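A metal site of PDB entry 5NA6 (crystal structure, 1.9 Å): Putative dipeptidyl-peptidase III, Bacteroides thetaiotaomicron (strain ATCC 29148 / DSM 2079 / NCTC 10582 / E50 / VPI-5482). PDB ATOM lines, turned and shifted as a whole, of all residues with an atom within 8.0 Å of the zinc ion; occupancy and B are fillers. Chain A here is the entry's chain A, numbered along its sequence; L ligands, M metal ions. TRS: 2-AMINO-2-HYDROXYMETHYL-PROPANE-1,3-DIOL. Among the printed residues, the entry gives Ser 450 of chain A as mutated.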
ATOM      1  N   THR A 445      10.031 -23.157 -19.043  1.00  0.00           N
ATOM      2  CA  THR A 445       9.957 -23.034 -17.591  1.00  0.00           C
ATOM      3  C   THR A 445      11.302 -23.284 -16.937  1.00  0.00           C
ATOM      4  O   THR A 445      11.701 -22.555 -16.015  1.00  0.00           O
ATOM      5  CB  THR A 445       8.909 -24.007 -17.052  1.00  0.00           C
ATOM      6  OG1 THR A 445       7.647 -23.678 -17.636  1.00  0.00           O
ATOM      7  CG2 THR A 445       8.826 -23.902 -15.540  1.00  0.00           C
ATOM      8  N   HIS A 448      13.520 -20.229 -17.560  1.00  0.00           N
ATOM      9  CA  HIS A 448      13.065 -19.131 -16.704  1.00  0.00           C
ATOM     10  C   HIS A 448      13.483 -19.355 -15.262  1.00  0.00           C
ATOM     11  O   HIS A 448      14.136 -18.500 -14.642  1.00  0.00           O
ATOM     12  CB  HIS A 448      11.537 -18.964 -16.848  1.00  0.00           C
ATOM     13  CG  HIS A 448      10.886 -18.085 -15.819  1.00  0.00           C
ATOM     14  ND1 HIS A 448       9.947 -17.138 -16.146  1.00  0.00           N
ATOM     15  CD2 HIS A 448      10.994 -18.051 -14.462  1.00  0.00           C
ATOM     16  CE1 HIS A 448       9.526 -16.526 -15.041  1.00  0.00           C
ATOM     17  NE2 HIS A 448      10.149 -17.061 -14.019  1.00  0.00           N
ATOM     18  N   GLU A 449      13.158 -20.519 -14.707  1.00  0.00           N
ATOM     19  CA  GLU A 449      13.324 -20.708 -13.270  1.00  0.00           C
ATOM     20  C   GLU A 449      14.763 -20.990 -12.872  1.00  0.00           C
ATOM     21  O   GLU A 449      15.196 -20.549 -11.790  1.00  0.00           O
ATOM     22  CB  GLU A 449      12.383 -21.806 -12.791  1.00  0.00           C
ATOM     23  CG  GLU A 449      10.943 -21.322 -12.861  1.00  0.00           C
ATOM     24  CD  GLU A 449       9.935 -22.322 -12.357  1.00  0.00           C
ATOM     25  OE1 GLU A 449      10.323 -23.467 -12.039  1.00  0.00           O
ATOM     26  OE2 GLU A 449       8.736 -21.948 -12.280  1.00  0.00           O
ATOM     27  N   SER A 450      15.543 -21.666 -13.695  1.00  0.00           N
ATOM     28  CA  SER A 450      16.881 -22.010 -13.236  1.00  0.00           C
ATOM     29  C   SER A 450      17.948 -21.010 -13.659  1.00  0.00           C
ATOM     30  O   SER A 450      18.998 -20.940 -13.006  1.00  0.00           O
ATOM     31  CB  SER A 450      17.278 -23.411 -13.713  1.00  0.00           C
ATOM     32  OG  SER A 450      17.564 -23.428 -15.092  1.00  0.00           O
ATOM     33  N   GLY A 452      16.917 -17.724 -15.666  1.00  0.00           N
ATOM     34  CA  GLY A 452      16.414 -16.418 -16.052  1.00  0.00           C
ATOM     35  C   GLY A 452      16.570 -15.381 -14.965  1.00  0.00           C
ATOM     36  O   GLY A 452      17.102 -14.292 -15.185  1.00  0.00           O
ATOM     37  N   HIS A 453      16.102 -15.704 -13.744  1.00  0.00           N
ATOM     38  CA  HIS A 453      16.240 -14.757 -12.643  1.00  0.00           C
ATOM     39  C   HIS A 453      17.684 -14.589 -12.221  1.00  0.00           C
ATOM     40  O   HIS A 453      18.085 -13.488 -11.825  1.00  0.00           O
ATOM     41  CB  HIS A 453      15.391 -15.193 -11.456  1.00  0.00           C
ATOM     42  CG  HIS A 453      13.915 -15.091 -11.699  1.00  0.00           C
ATOM     43  ND1 HIS A 453      13.267 -13.885 -11.881  1.00  0.00           N
ATOM     44  CD2 HIS A 453      12.958 -16.054 -11.755  1.00  0.00           C
ATOM     45  CE1 HIS A 453      11.976 -14.104 -12.064  1.00  0.00           C
ATOM     46  NE2 HIS A 453      11.762 -15.414 -11.994  1.00  0.00           N
ATOM     47  N   SER A 472       7.992  -6.582  -9.896  1.00  0.00           N
ATOM     48  CA  SER A 472       7.676  -7.997 -10.123  1.00  0.00           C
ATOM     49  C   SER A 472       7.307  -8.269 -11.568  1.00  0.00           C
ATOM     50  O   SER A 472       7.735  -9.275 -12.150  1.00  0.00           O
ATOM     51  CB  SER A 472       6.537  -8.453  -9.210  1.00  0.00           C
ATOM     52  OG  SER A 472       6.970  -8.422  -7.859  1.00  0.00           O
ATOM     53  N   GLU A 475      10.476  -8.079 -13.640  1.00  0.00           N
ATOM     54  CA  GLU A 475      11.391  -9.170 -13.335  1.00  0.00           C
ATOM     55  C   GLU A 475      10.889 -10.509 -13.908  1.00  0.00           C
ATOM     56  O   GLU A 475      11.689 -11.288 -14.444  1.00  0.00           O
ATOM     57  CB  GLU A 475      11.617  -9.248 -11.813  1.00  0.00           C
ATOM     58  CG  GLU A 475      12.533 -10.403 -11.341  1.00  0.00           C
ATOM     59  CD  GLU A 475      13.909 -10.399 -12.014  1.00  0.00           C
ATOM     60  OE1 GLU A 475      14.542 -11.479 -12.060  1.00  0.00           O
ATOM     61  OE2 GLU A 475      14.366  -9.333 -12.491  1.00  0.00           O
ATOM     62  N   GLU A 476       9.581 -10.790 -13.825  1.00  0.00           N
ATOM     63  CA  GLU A 476       9.076 -12.015 -14.439  1.00  0.00           C
ATOM     64  C   GLU A 476       9.131 -11.941 -15.969  1.00  0.00           C
ATOM     65  O   GLU A 476       9.461 -12.937 -16.629  1.00  0.00           O
ATOM     66  CB  GLU A 476       7.662 -12.340 -13.957  1.00  0.00           C
ATOM     67  CG  GLU A 476       7.535 -12.539 -12.463  1.00  0.00           C
ATOM     68  CD  GLU A 476       8.391 -13.698 -11.922  1.00  0.00           C
ATOM     69  OE1 GLU A 476       8.781 -14.583 -12.698  1.00  0.00           O
ATOM     70  OE2 GLU A 476       8.672 -13.703 -10.718  1.00  0.00           O
ATOM     71  N   ALA A 477       8.847 -10.766 -16.555  1.00  0.00           N
ATOM     72  CA  ALA A 477       9.044 -10.581 -17.996  1.00  0.00           C
ATOM     73  C   ALA A 477      10.506 -10.860 -18.397  1.00  0.00           C
ATOM     74  O   ALA A 477      10.767 -11.485 -19.431  1.00  0.00           O
ATOM     75  CB  ALA A 477       8.668  -9.155 -18.405  1.00  0.00           C
ATOM     76  N   ARG A 478      11.446 -10.381 -17.588  1.00  0.00           N
ATOM     77  CA  ARG A 478      12.867 -10.586 -17.879  1.00  0.00           C
ATOM     78  C   ARG A 478      13.211 -12.066 -17.917  1.00  0.00           C
ATOM     79  O   ARG A 478      13.897 -12.552 -18.842  1.00  0.00           O
ATOM     80  CB  ARG A 478      13.703  -9.878 -16.811  1.00  0.00           C
ATOM     81  CG  ARG A 478      15.198  -9.691 -17.144  1.00  0.00           C
ATOM     82  CD  ARG A 478      15.957  -8.960 -16.020  1.00  0.00           C
ATOM     83  NE  ARG A 478      16.074  -9.785 -14.815  1.00  0.00           N
ATOM     84  CZ  ARG A 478      17.027 -10.704 -14.632  1.00  0.00           C
ATOM     85  NH1 ARG A 478      17.950 -10.898 -15.579  1.00  0.00           N
ATOM     86  NH2 ARG A 478      17.041 -11.426 -13.517  1.00  0.00           N
ATOM     87  N   ALA A 479      12.774 -12.805 -16.899  1.00  0.00           N
ATOM     88  CA  ALA A 479      13.059 -14.237 -16.854  1.00  0.00           C
ATOM     89  C   ALA A 479      12.350 -14.958 -17.988  1.00  0.00           C
ATOM     90  O   ALA A 479      12.910 -15.876 -18.599  1.00  0.00           O
ATOM     91  CB  ALA A 479      12.659 -14.817 -15.501  1.00  0.00           C
ATOM     92  N   ASP A 480      11.099 -14.564 -18.296  1.00  0.00           N
ATOM     93  CA  ASP A 480      10.380 -15.187 -19.412  1.00  0.00           C
ATOM     94  C   ASP A 480      11.102 -14.962 -20.736  1.00  0.00           C
ATOM     95  O   ASP A 480      11.197 -15.876 -21.574  1.00  0.00           O
ATOM     96  CB  ASP A 480       8.957 -14.629 -19.492  1.00  0.00           C
ATOM     97  CG  ASP A 480       7.957 -15.529 -18.817  1.00  0.00           C
ATOM     98  OD1 ASP A 480       8.365 -16.568 -18.243  1.00  0.00           O
ATOM     99  OD2 ASP A 480       6.750 -15.162 -18.863  1.00  0.00           O
ATOM    100  N   HIS A 533       2.236 -11.892 -13.375  1.00  0.00           N
ATOM    101  CA  HIS A 533       2.606 -12.781 -14.466  1.00  0.00           C
ATOM    102  C   HIS A 533       1.728 -12.539 -15.694  1.00  0.00           C
ATOM    103  O   HIS A 533       2.234 -12.482 -16.821  1.00  0.00           O
ATOM    104  CB  HIS A 533       2.548 -14.254 -14.028  1.00  0.00           C
ATOM    105  CG  HIS A 533       3.634 -14.654 -13.057  1.00  0.00           C
ATOM    106  ND1 HIS A 533       4.837 -15.193 -13.458  1.00  0.00           N
ATOM    107  CD2 HIS A 533       3.697 -14.565 -11.710  1.00  0.00           C
ATOM    108  CE1 HIS A 533       5.591 -15.429 -12.408  1.00  0.00           C
ATOM    109  NE2 HIS A 533       4.927 -15.055 -11.326  1.00  0.00           N
ATOM    110  N   ASN A 536       3.025  -9.620 -17.326  1.00  0.00           N
ATOM    111  CA  ASN A 536       4.309  -9.767 -17.986  1.00  0.00           C
ATOM    112  C   ASN A 536       4.147 -10.499 -19.303  1.00  0.00           C
ATOM    113  O   ASN A 536       4.871 -10.214 -20.273  1.00  0.00           O
ATOM    114  CB  ASN A 536       5.347 -10.451 -17.045  1.00  0.00           C
ATOM    115  CG  ASN A 536       5.559 -11.982 -17.310  1.00  0.00           C
ATOM    116  OD1 ASN A 536       5.332 -12.792 -16.419  1.00  0.00           O
ATOM    117  ND2 ASN A 536       6.083 -12.340 -18.481  1.00  0.00           N
HETATM  118  C   TRS L   1       8.679 -17.032  -9.629  1.00  0.00           C
HETATM  119  C1  TRS L   1       7.947 -17.564 -10.866  1.00  0.00           C
HETATM  120  C2  TRS L   1       9.532 -18.143  -9.012  1.00  0.00           C
HETATM  121  C3  TRS L   1       7.633 -16.496  -8.654  1.00  0.00           C
HETATM  122  N   TRS L   1       9.548 -15.910  -9.993  1.00  0.00           N
HETATM  123  O1  TRS L   1       6.943 -18.460 -10.438  1.00  0.00           O
HETATM  124  O2  TRS L   1      10.547 -18.558  -9.922  1.00  0.00           O
HETATM  125  O3  TRS L   1       6.784 -15.588  -9.337  1.00  0.00           O
HETATM  126 ZN    ZN M   1       9.919 -16.340 -12.066  1.00  0.00          ZN
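The backbone carbonyl oxygen (O) of His 453 is in hydrogen-bond range of the guanidinium group (NH2) of Arg 478 (2.9 Å).
OD1 of Asp 480 is in hydrogen-bond range of ND1 of His 448.
ND1 of His 453 is in hydrogen-bond range of OE1 of Glu 475 (2.7 Å).
Within 4 Å of the zinc ion: His 448, His 453 and Glu 476.
The zinc ion is bound by NE2 of His 453 (2.1 Å), NE2 of His 448 (2.1 Å), N of the ligand (2.1 Å) and OE1 of Glu 476 (2.2 Å).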
